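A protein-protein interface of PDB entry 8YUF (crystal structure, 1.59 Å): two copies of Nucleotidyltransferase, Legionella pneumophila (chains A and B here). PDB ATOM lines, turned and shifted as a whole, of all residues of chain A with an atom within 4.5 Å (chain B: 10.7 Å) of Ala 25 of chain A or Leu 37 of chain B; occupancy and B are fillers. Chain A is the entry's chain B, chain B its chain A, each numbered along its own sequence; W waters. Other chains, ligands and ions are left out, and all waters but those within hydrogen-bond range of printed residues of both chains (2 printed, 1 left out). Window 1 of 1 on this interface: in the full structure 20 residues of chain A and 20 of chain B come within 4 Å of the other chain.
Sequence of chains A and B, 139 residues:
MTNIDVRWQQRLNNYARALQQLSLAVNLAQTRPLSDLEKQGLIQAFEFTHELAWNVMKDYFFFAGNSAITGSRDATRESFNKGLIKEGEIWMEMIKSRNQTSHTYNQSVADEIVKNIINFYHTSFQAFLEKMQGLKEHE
Among the printed residues, merely in contact across the chains: Gln 21 of chain A with Gln 40 of chain B, Ala 25 of chain A with Leu 37 of chain B, Leu 28 of chain A with Leu 37 of chain B, Glu 38 of chain A with Leu 37 of chain B, Gly 41 of chain A with Leu 37 of chain B, Gly 41 of chain A with Gln 40 of chain B, Gly 41 of chain A with Gly 41 of chain B and Leu 42 of chain A with Leu 37 of chain B.
OE1 of Gln 21 of chain A lies close to O of Tyr 105 of chain B (3.3 Å).
No residue of chain B comes within 4 Å of Leu 24 of chain A.
Ala 25 of chain A touches one residue of chain B.
Asn 27 of chain A touches none of the printed residues of chain B.
No residue of chain B comes within 4 Å of Ala 29 of chain A.
Printed residues of chain B within 4 Å of Glu 38 of chain A: Leu 37 (3.9 Å).
Of chain B, only Leu 37 (3.5 Å), Gln 40 (3.6 Å) and Gly 41 (3.2 Å) come within 4 Å of Gly 41 of chain A.
Printed residues of chain B within 4 Å of Leu 42 of chain A: Leu 37 (3.6 Å).
Pro 33 of chain B touches none of the printed residues of chain A.
Printed residues of chain A within 4 Å of Tyr 105 of chain B: Gln 21 (3.3 Å).
The nearest residue of chain B that does not touch Ala 25 of chain A is Gln 40 of chain B (7.9 Å).
Printed residues of chain A that touch a printed residue of chain B: Gln 21, Ala 25, Leu 28, Glu 38, Gly 41 and Leu 42.
Among the printed residues, 9 pairs touch across the chains.
Gly 41 of chain B touches its own counterpart, Gly 41 of chain A.
Positions printed for both chains: 25, 28, 38, 41 and 42.
Water W2 bridges OE2 of Glu 38 of chain A and OG of Ser 35 of chain B.
Water W1 lies within hydrogen-bond range of OE2 of Glu 38 of chain A and OE2 of Glu 38 of chain B.
OG of Ser 35 of chain B lies close to N of Leu 37 of chain B (3.3 Å).
The side-chain amide oxygen (OE1) of Gln 40 of chain B is in hydrogen-bond range of the side-chain hydroxyl (OG1) of Thr 104 of chain B (2.8 Å).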
ATOM      1  N   GLN A  21     -16.871 -27.824   3.412  1.00  0.00           N
ATOM      2  CA  GLN A  21     -17.330 -26.444   3.290  1.00  0.00           C
ATOM      3  C   GLN A  21     -18.788 -26.386   2.838  1.00  0.00           C
ATOM      4  O   GLN A  21     -19.559 -25.545   3.308  1.00  0.00           O
ATOM      5  CB  GLN A  21     -16.426 -25.675   2.323  1.00  0.00           C
ATOM      6  CG  GLN A  21     -16.760 -24.193   2.242  1.00  0.00           C
ATOM      7  CD  GLN A  21     -15.651 -23.365   1.610  1.00  0.00           C
ATOM      8  OE1 GLN A  21     -14.533 -23.858   1.391  1.00  0.00           O
ATOM      9  NE2 GLN A  21     -15.946 -22.076   1.349  1.00  0.00           N
ATOM     10  N   LEU A  22     -19.192 -27.267   1.923  1.00  0.00           N
ATOM     11  CA  LEU A  22     -20.604 -27.316   1.568  1.00  0.00           C
ATOM     12  C   LEU A  22     -21.461 -27.656   2.784  1.00  0.00           C
ATOM     13  O   LEU A  22     -22.539 -27.087   2.958  1.00  0.00           O
ATOM     14  CB  LEU A  22     -20.838 -28.309   0.431  1.00  0.00           C
ATOM     15  CG  LEU A  22     -22.279 -28.576   0.046  1.00  0.00           C
ATOM     16  CD1 LEU A  22     -22.921 -27.351  -0.528  1.00  0.00           C
ATOM     17  CD2 LEU A  22     -22.313 -29.760  -0.986  1.00  0.00           C
ATOM     18  N   SER A  23     -21.006 -28.595   3.621  1.00  0.00           N
ATOM     19  CA  SER A  23     -21.757 -28.988   4.809  1.00  0.00           C
ATOM     20  C   SER A  23     -21.961 -27.818   5.755  1.00  0.00           C
ATOM     21  O   SER A  23     -23.030 -27.691   6.367  1.00  0.00           O
ATOM     22  CB  SER A  23     -21.028 -30.111   5.538  1.00  0.00           C
ATOM     23  OG  SER A  23     -20.977 -31.284   4.773  1.00  0.00           O
ATOM     24  N   LEU A  24     -20.952 -26.958   5.890  1.00  0.00           N
ATOM     25  CA  LEU A  24     -21.107 -25.775   6.731  1.00  0.00           C
ATOM     26  C   LEU A  24     -22.303 -24.946   6.291  1.00  0.00           C
ATOM     27  O   LEU A  24     -23.147 -24.574   7.116  1.00  0.00           O
ATOM     28  CB  LEU A  24     -19.848 -24.922   6.717  1.00  0.00           C
ATOM     29  CG  LEU A  24     -18.567 -25.602   7.206  1.00  0.00           C
ATOM     30  CD1 LEU A  24     -17.362 -24.690   7.040  1.00  0.00           C
ATOM     31  CD2 LEU A  24     -18.707 -26.050   8.619  1.00  0.00           C
ATOM     32  N   ALA A  25     -22.425 -24.710   4.980  1.00  0.00           N
ATOM     33  CA  ALA A  25     -23.499 -23.874   4.460  1.00  0.00           C
ATOM     34  C   ALA A  25     -24.838 -24.579   4.589  1.00  0.00           C
ATOM     35  O   ALA A  25     -25.862 -23.935   4.850  1.00  0.00           O
ATOM     36  CB  ALA A  25     -23.217 -23.508   2.999  1.00  0.00           C
ATOM     37  N   VAL A  26     -24.851 -25.908   4.391  1.00  0.00           N
ATOM     38  CA  VAL A  26     -26.096 -26.658   4.480  1.00  0.00           C
ATOM     39  C   VAL A  26     -26.599 -26.654   5.912  1.00  0.00           C
ATOM     40  O   VAL A  26     -27.784 -26.451   6.156  1.00  0.00           O
ATOM     41  CB  VAL A  26     -25.908 -28.093   3.958  1.00  0.00           C
ATOM     42  CG1 VAL A  26     -27.076 -28.937   4.363  1.00  0.00           C
ATOM     43  CG2 VAL A  26     -25.697 -28.102   2.459  1.00  0.00           C
ATOM     44  N   ASN A  27     -25.693 -26.801   6.881  1.00  0.00           N
ATOM     45  CA  ASN A  27     -26.058 -26.666   8.289  1.00  0.00           C
ATOM     46  C   ASN A  27     -26.532 -25.252   8.624  1.00  0.00           C
ATOM     47  O   ASN A  27     -27.512 -25.088   9.364  1.00  0.00           O
ATOM     48  CB  ASN A  27     -24.869 -27.028   9.179  1.00  0.00           C
ATOM     49  CG  ASN A  27     -24.388 -28.447   8.978  1.00  0.00           C
ATOM     50  OD1 ASN A  27     -24.935 -29.201   8.185  1.00  0.00           O
ATOM     51  ND2 ASN A  27     -23.312 -28.799   9.673  1.00  0.00           N
ATOM     52  N   LEU A  28     -25.860 -24.221   8.081  1.00  0.00           N
ATOM     53  CA  LEU A  28     -26.295 -22.848   8.334  1.00  0.00           C
ATOM     54  C   LEU A  28     -27.745 -22.638   7.926  1.00  0.00           C
ATOM     55  O   LEU A  28     -28.508 -21.978   8.639  1.00  0.00           O
ATOM     56  CB  LEU A  28     -25.403 -21.867   7.595  1.00  0.00           C
ATOM     57  CG  LEU A  28     -25.785 -20.394   7.747  1.00  0.00           C
ATOM     58  CD1 LEU A  28     -25.586 -19.928   9.181  1.00  0.00           C
ATOM     59  CD2 LEU A  28     -24.931 -19.553   6.765  1.00  0.00           C
ATOM     60  N   ALA A  29     -28.144 -23.220   6.801  1.00  0.00           N
ATOM     61  CA  ALA A  29     -29.511 -23.062   6.321  1.00  0.00           C
ATOM     62  C   ALA A  29     -30.539 -23.658   7.273  1.00  0.00           C
ATOM     63  O   ALA A  29     -31.718 -23.283   7.207  1.00  0.00           O
ATOM     64  CB  ALA A  29     -29.668 -23.692   4.936  1.00  0.00           C
ATOM     65  N   GLU A  38     -25.916 -15.486   0.014  1.00  0.00           N
ATOM     66  CA  GLU A  38     -25.550 -16.798   0.536  1.00  0.00           C
ATOM     67  C   GLU A  38     -26.049 -17.955  -0.326  1.00  0.00           C
ATOM     68  O   GLU A  38     -25.375 -18.986  -0.411  1.00  0.00           O
ATOM     69  CB  GLU A  38     -26.071 -16.930   1.955  1.00  0.00           C
ATOM     70  CG  GLU A  38     -25.320 -16.063   2.966  1.00  0.00           C
ATOM     71  CD  GLU A  38     -25.955 -16.031   4.329  1.00  0.00           C
ATOM     72  OE1 GLU A  38     -27.207 -16.082   4.426  1.00  0.00           O
ATOM     73  OE2 GLU A  38     -25.186 -15.907   5.316  1.00  0.00           O
ATOM     74  N   GLY A  41     -23.640 -18.454  -2.968  1.00  0.00           N
ATOM     75  CA  GLY A  41     -22.488 -19.159  -2.415  1.00  0.00           C
ATOM     76  C   GLY A  41     -22.717 -20.650  -2.199  1.00  0.00           C
ATOM     77  O   GLY A  41     -21.807 -21.452  -2.400  1.00  0.00           O
ATOM     78  N   LEU A  42     -23.935 -21.034  -1.805  1.00  0.00           N
ATOM     79  CA  LEU A  42     -24.260 -22.445  -1.645  1.00  0.00           C
ATOM     80  C   LEU A  42     -24.189 -23.145  -2.992  1.00  0.00           C
ATOM     81  O   LEU A  42     -23.721 -24.286  -3.086  1.00  0.00           O
ATOM     82  CB  LEU A  42     -25.659 -22.585  -1.036  1.00  0.00           C
ATOM     83  CG  LEU A  42     -26.100 -24.019  -0.756  1.00  0.00           C
ATOM     84  CD1 LEU A  42     -25.320 -24.613   0.397  1.00  0.00           C
ATOM     85  CD2 LEU A  42     -27.604 -24.117  -0.452  1.00  0.00           C
ATOM     86  N   ALA B  25     -23.781  -7.016  -4.057  1.00  0.00           N
ATOM     87  CA  ALA B  25     -22.814  -7.704  -3.208  1.00  0.00           C
ATOM     88  C   ALA B  25     -21.543  -6.876  -3.062  1.00  0.00           C
ATOM     89  O   ALA B  25     -20.908  -6.852  -1.996  1.00  0.00           O
ATOM     90  CB  ALA B  25     -22.508  -9.072  -3.805  1.00  0.00           C
ATOM     91  N   LEU B  28     -22.332  -4.276  -0.532  1.00  0.00           N
ATOM     92  CA  LEU B  28     -22.380  -4.893   0.786  1.00  0.00           C
ATOM     93  C   LEU B  28     -20.981  -5.035   1.351  1.00  0.00           C
ATOM     94  O   LEU B  28     -20.767  -4.826   2.547  1.00  0.00           O
ATOM     95  CB  LEU B  28     -23.060  -6.261   0.708  1.00  0.00           C
ATOM     96  CG  LEU B  28     -23.109  -7.015   2.029  1.00  0.00           C
ATOM     97  CD1 LEU B  28     -24.061  -6.347   3.030  1.00  0.00           C
ATOM     98  CD2 LEU B  28     -23.568  -8.483   1.765  1.00  0.00           C
ATOM     99  N   ARG B  32     -19.252  -4.116   5.472  1.00  0.00           N
ATOM    100  CA  ARG B  32     -18.689  -5.052   6.427  1.00  0.00           C
ATOM    101  C   ARG B  32     -17.920  -6.132   5.656  1.00  0.00           C
ATOM    102  O   ARG B  32     -18.125  -6.306   4.456  1.00  0.00           O
ATOM    103  CB  ARG B  32     -19.784  -5.689   7.288  1.00  0.00           C
ATOM    104  CG  ARG B  32     -20.876  -6.421   6.457  1.00  0.00           C
ATOM    105  CD  ARG B  32     -21.727  -7.334   7.351  1.00  0.00           C
ATOM    106  NE  ARG B  32     -22.841  -7.916   6.605  1.00  0.00           N
ATOM    107  CZ  ARG B  32     -22.743  -9.006   5.847  1.00  0.00           C
ATOM    108  NH1 ARG B  32     -21.597  -9.657   5.708  1.00  0.00           N
ATOM    109  NH2 ARG B  32     -23.824  -9.466   5.214  1.00  0.00           N
ATOM    110  N   PRO B  33     -17.058  -6.870   6.327  1.00  0.00           N
ATOM    111  CA  PRO B  33     -16.447  -8.031   5.687  1.00  0.00           C
ATOM    112  C   PRO B  33     -17.488  -9.063   5.282  1.00  0.00           C
ATOM    113  O   PRO B  33     -18.490  -9.269   5.976  1.00  0.00           O
ATOM    114  CB  PRO B  33     -15.519  -8.582   6.771  1.00  0.00           C
ATOM    115  CG  PRO B  33     -15.368  -7.517   7.731  1.00  0.00           C
ATOM    116  CD  PRO B  33     -16.624  -6.722   7.720  1.00  0.00           C
ATOM    117  N   LEU B  34     -17.243  -9.713   4.141  1.00  0.00           N
ATOM    118  CA  LEU B  34     -18.091 -10.825   3.715  1.00  0.00           C
ATOM    119  C   LEU B  34     -17.695 -12.109   4.443  1.00  0.00           C
ATOM    120  O   LEU B  34     -16.510 -12.375   4.673  1.00  0.00           O
ATOM    121  CB  LEU B  34     -18.020 -11.040   2.195  1.00  0.00           C
ATOM    122  CG  LEU B  34     -18.407  -9.825   1.317  1.00  0.00           C
ATOM    123  CD1 LEU B  34     -18.248 -10.142  -0.161  1.00  0.00           C
ATOM    124  CD2 LEU B  34     -19.836  -9.373   1.641  1.00  0.00           C
ATOM    125  N   SER B  35     -18.693 -12.911   4.801  1.00  0.00           N
ATOM    126  CA  SER B  35     -18.420 -14.264   5.261  1.00  0.00           C
ATOM    127  C   SER B  35     -17.811 -15.126   4.142  1.00  0.00           C
ATOM    128  O   SER B  35     -17.869 -14.800   2.947  1.00  0.00           O
ATOM    129  CB  SER B  35     -19.697 -14.910   5.755  1.00  0.00           C
ATOM    130  OG  SER B  35     -20.484 -15.256   4.617  1.00  0.00           O
ATOM    131  N   ASP B  36     -17.255 -16.279   4.540  1.00  0.00           N
ATOM    132  CA  ASP B  36     -16.719 -17.203   3.551  1.00  0.00           C
ATOM    133  C   ASP B  36     -17.804 -17.588   2.560  1.00  0.00           C
ATOM    134  O   ASP B  36     -17.572 -17.672   1.351  1.00  0.00           O
ATOM    135  CB  ASP B  36     -16.162 -18.444   4.238  1.00  0.00           C
ATOM    136  CG  ASP B  36     -14.831 -18.191   4.941  1.00  0.00           C
ATOM    137  OD1 ASP B  36     -14.234 -17.110   4.746  1.00  0.00           O
ATOM    138  OD2 ASP B  36     -14.368 -19.107   5.682  1.00  0.00           O
ATOM    139  N   LEU B  37     -19.009 -17.805   3.050  1.00  0.00           N
ATOM    140  CA  LEU B  37     -20.066 -18.215   2.121  1.00  0.00           C
ATOM    141  C   LEU B  37     -20.462 -17.081   1.167  1.00  0.00           C
ATOM    142  O   LEU B  37     -20.752 -17.296  -0.028  1.00  0.00           O
ATOM    143  CB  LEU B  37     -21.277 -18.697   2.909  1.00  0.00           C
ATOM    144  CG  LEU B  37     -22.439 -19.235   2.110  1.00  0.00           C
ATOM    145  CD1 LEU B  37     -22.053 -20.374   1.178  1.00  0.00           C
ATOM    146  CD2 LEU B  37     -23.567 -19.708   3.051  1.00  0.00           C
ATOM    147  N   GLU B  38     -20.530 -15.869   1.704  1.00  0.00           N
ATOM    148  CA  GLU B  38     -20.842 -14.729   0.876  1.00  0.00           C
ATOM    149  C   GLU B  38     -19.774 -14.494  -0.171  1.00  0.00           C
ATOM    150  O   GLU B  38     -20.098 -14.021  -1.261  1.00  0.00           O
ATOM    151  CB  GLU B  38     -21.000 -13.496   1.751  1.00  0.00           C
ATOM    152  CG  GLU B  38     -22.288 -13.472   2.572  1.00  0.00           C
ATOM    153  CD  GLU B  38     -22.367 -12.340   3.589  1.00  0.00           C
ATOM    154  OE1 GLU B  38     -21.313 -11.940   4.153  1.00  0.00           O
ATOM    155  OE2 GLU B  38     -23.499 -11.897   3.859  1.00  0.00           O
ATOM    156  N   LYS B  39     -18.498 -14.755   0.165  1.00  0.00           N
ATOM    157  CA  LYS B  39     -17.422 -14.672  -0.816  1.00  0.00           C
ATOM    158  C   LYS B  39     -17.687 -15.625  -1.977  1.00  0.00           C
ATOM    159  O   LYS B  39     -17.491 -15.271  -3.152  1.00  0.00           O
ATOM    160  CB  LYS B  39     -16.075 -14.990  -0.161  1.00  0.00           C
ATOM    161  CG  LYS B  39     -15.468 -13.837   0.553  1.00  0.00           C
ATOM    162  CD  LYS B  39     -14.145 -14.274   1.234  1.00  0.00           C
ATOM    163  CE  LYS B  39     -14.031 -13.831   2.656  1.00  0.00           C
ATOM    164  NZ  LYS B  39     -12.652 -13.989   3.162  1.00  0.00           N
ATOM    165  N   GLN B  40     -18.125 -16.847  -1.658  1.00  0.00           N
ATOM    166  CA  GLN B  40     -18.479 -17.793  -2.699  1.00  0.00           C
ATOM    167  C   GLN B  40     -19.609 -17.238  -3.539  1.00  0.00           C
ATOM    168  O   GLN B  40     -19.623 -17.429  -4.761  1.00  0.00           O
ATOM    169  CB  GLN B  40     -18.844 -19.138  -2.084  1.00  0.00           C
ATOM    170  CG  GLN B  40     -17.713 -19.796  -1.298  1.00  0.00           C
ATOM    171  CD  GLN B  40     -16.472 -20.118  -2.127  1.00  0.00           C
ATOM    172  OE1 GLN B  40     -16.541 -20.471  -3.292  1.00  0.00           O
ATOM    173  NE2 GLN B  40     -15.319 -20.018  -1.492  1.00  0.00           N
ATOM    174  N   GLY B  41     -20.567 -16.560  -2.907  1.00  0.00           N
ATOM    175  CA  GLY B  41     -21.699 -16.024  -3.652  1.00  0.00           C
ATOM    176  C   GLY B  41     -21.291 -14.853  -4.533  1.00  0.00           C
ATOM    177  O   GLY B  41     -21.798 -14.692  -5.643  1.00  0.00           O
ATOM    178  N   LEU B  42     -20.335 -14.059  -4.062  1.00  0.00           N
ATOM    179  CA  LEU B  42     -19.793 -12.987  -4.883  1.00  0.00           C
ATOM    180  C   LEU B  42     -19.105 -13.560  -6.112  1.00  0.00           C
ATOM    181  O   LEU B  42     -19.197 -12.986  -7.199  1.00  0.00           O
ATOM    182  CB  LEU B  42     -18.820 -12.132  -4.064  1.00  0.00           C
ATOM    183  CG  LEU B  42     -18.266 -10.939  -4.819  1.00  0.00           C
ATOM    184  CD1 LEU B  42     -19.237  -9.827  -5.001  1.00  0.00           C
ATOM    185  CD2 LEU B  42     -17.049 -10.394  -4.030  1.00  0.00           C
ATOM    186  N   ILE B  43     -18.388 -14.681  -5.963  1.00  0.00           N
ATOM    187  CA  ILE B  43     -17.725 -15.304  -7.110  1.00  0.00           C
ATOM    188  C   ILE B  43     -18.746 -15.841  -8.112  1.00  0.00           C
ATOM    189  O   ILE B  43     -18.612 -15.622  -9.321  1.00  0.00           O
ATOM    190  CB  ILE B  43     -16.783 -16.417  -6.624  1.00  0.00           C
ATOM    191  CG1 ILE B  43     -15.668 -15.802  -5.825  1.00  0.00           C
ATOM    192  CG2 ILE B  43     -16.310 -17.281  -7.788  1.00  0.00           C
ATOM    193  CD1 ILE B  43     -14.972 -16.853  -4.927  1.00  0.00           C
ATOM    194  N   GLN B  44     -19.796 -16.519  -7.622  1.00  0.00           N
ATOM    195  CA  GLN B  44     -20.880 -16.980  -8.495  1.00  0.00           C
ATOM    196  C   GLN B  44     -21.523 -15.826  -9.256  1.00  0.00           C
ATOM    197  O   GLN B  44     -21.814 -15.967 -10.451  1.00  0.00           O
ATOM    198  CB  GLN B  44     -21.936 -17.742  -7.690  1.00  0.00           C
ATOM    199  CG  GLN B  44     -23.136 -18.177  -8.470  1.00  0.00           C
ATOM    200  CD  GLN B  44     -22.839 -19.231  -9.510  1.00  0.00           C
ATOM    201  OE1 GLN B  44     -21.770 -19.877  -9.518  1.00  0.00           O
ATOM    202  NE2 GLN B  44     -23.814 -19.452 -10.373  1.00  0.00           N
ATOM    203  N   ALA B  45     -21.787 -14.696  -8.596  1.00  0.00           N
ATOM    204  CA  ALA B  45     -22.325 -13.522  -9.311  1.00  0.00           C
ATOM    205  C   ALA B  45     -21.346 -12.977 -10.354  1.00  0.00           C
ATOM    206  O   ALA B  45     -21.749 -12.562 -11.456  1.00  0.00           O
ATOM    207  CB  ALA B  45     -22.677 -12.428  -8.323  1.00  0.00           C
ATOM    208  N   THR B 104     -12.084 -22.791  -5.526  1.00  0.00           N
ATOM    209  CA  THR B 104     -12.384 -21.755  -4.551  1.00  0.00           C
ATOM    210  C   THR B 104     -12.712 -22.286  -3.160  1.00  0.00           C
ATOM    211  O   THR B 104     -12.943 -21.477  -2.267  1.00  0.00           O
ATOM    212  CB  THR B 104     -13.507 -20.853  -5.065  1.00  0.00           C
ATOM    213  OG1 THR B 104     -14.738 -21.568  -5.191  1.00  0.00           O
ATOM    214  CG2 THR B 104     -13.137 -20.269  -6.426  1.00  0.00           C
ATOM    215  N   TYR B 105     -12.690 -23.598  -2.922  1.00  0.00           N
ATOM    216  CA  TYR B 105     -12.739 -24.117  -1.560  1.00  0.00           C
ATOM    217  C   TYR B 105     -11.417 -23.892  -0.838  1.00  0.00           C
ATOM    218  O   TYR B 105     -11.347 -24.075   0.381  1.00  0.00           O
ATOM    219  CB  TYR B 105     -13.125 -25.625  -1.569  1.00  0.00           C
ATOM    220  CG  TYR B 105     -12.178 -26.548  -2.339  1.00  0.00           C
ATOM    221  CD1 TYR B 105     -12.309 -26.762  -3.684  1.00  0.00           C
ATOM    222  CD2 TYR B 105     -11.175 -27.218  -1.696  1.00  0.00           C
ATOM    223  CE1 TYR B 105     -11.453 -27.562  -4.369  1.00  0.00           C
ATOM    224  CE2 TYR B 105     -10.356 -28.044  -2.372  1.00  0.00           C
ATOM    225  CZ  TYR B 105     -10.482 -28.203  -3.706  1.00  0.00           C
ATOM    226  OH  TYR B 105      -9.623 -29.008  -4.385  1.00  0.00           O
ATOM    227  N   GLN B 107      -9.284 -21.111   0.555  1.00  0.00           N
ATOM    228  CA  GLN B 107      -9.585 -19.719   0.875  1.00  0.00           C
ATOM    229  C   GLN B 107      -8.649 -18.749   0.160  1.00  0.00           C
ATOM    230  O   GLN B 107      -9.077 -17.637  -0.186  1.00  0.00           O
ATOM    231  CB  GLN B 107      -9.521 -19.491   2.383  1.00  0.00           C
ATOM    232  CG  GLN B 107     -10.292 -18.239   2.833  1.00  0.00           C
ATOM    233  CD  GLN B 107     -11.744 -18.265   2.405  1.00  0.00           C
ATOM    234  OE1 GLN B 107     -12.433 -19.255   2.606  1.00  0.00           O
ATOM    235  NE2 GLN B 107     -12.207 -17.190   1.780  1.00  0.00           N
ATOM    236  N   ALA B 110     -10.243 -18.198  -3.278  1.00  0.00           N
ATOM    237  CA  ALA B 110     -11.457 -17.403  -3.173  1.00  0.00           C
ATOM    238  C   ALA B 110     -11.111 -15.941  -2.882  1.00  0.00           C
ATOM    239  O   ALA B 110     -11.651 -15.017  -3.503  1.00  0.00           O
ATOM    240  CB  ALA B 110     -12.352 -17.975  -2.072  1.00  0.00           C
ATOM    241  N   ASP B 111     -10.220 -15.707  -1.914  1.00  0.00           N
ATOM    242  CA  ASP B 111      -9.858 -14.331  -1.550  1.00  0.00           C
ATOM    243  C   ASP B 111      -9.258 -13.548  -2.731  1.00  0.00           C
ATOM    244  O   ASP B 111      -9.503 -12.334  -2.873  1.00  0.00           O
ATOM    245  CB  ASP B 111      -8.883 -14.354  -0.383  1.00  0.00           C
ATOM    246  CG  ASP B 111      -9.522 -14.705   0.880  1.00  0.00           C
ATOM    247  OD1 ASP B 111     -10.769 -14.763   0.945  1.00  0.00           O
ATOM    248  OD2 ASP B 111      -8.783 -14.938   1.846  1.00  0.00           O
ATOM    249  N   VAL B 114     -12.102 -12.674  -5.203  1.00  0.00           N
ATOM    250  CA  VAL B 114     -12.913 -11.623  -4.570  1.00  0.00           C
ATOM    251  C   VAL B 114     -12.216 -10.256  -4.655  1.00  0.00           C
ATOM    252  O   VAL B 114     -12.834  -9.234  -4.988  1.00  0.00           O
ATOM    253  CB  VAL B 114     -13.220 -11.985  -3.107  1.00  0.00           C
ATOM    254  CG1 VAL B 114     -13.748 -10.791  -2.358  1.00  0.00           C
ATOM    255  CG2 VAL B 114     -14.219 -13.145  -3.028  1.00  0.00           C
HETATM  256  O   HOH W   1     -24.953 -13.065   6.286  1.00  0.00           O
HETATM  257  O   HOH W   2     -22.604 -16.350   5.862  1.00  0.00           O
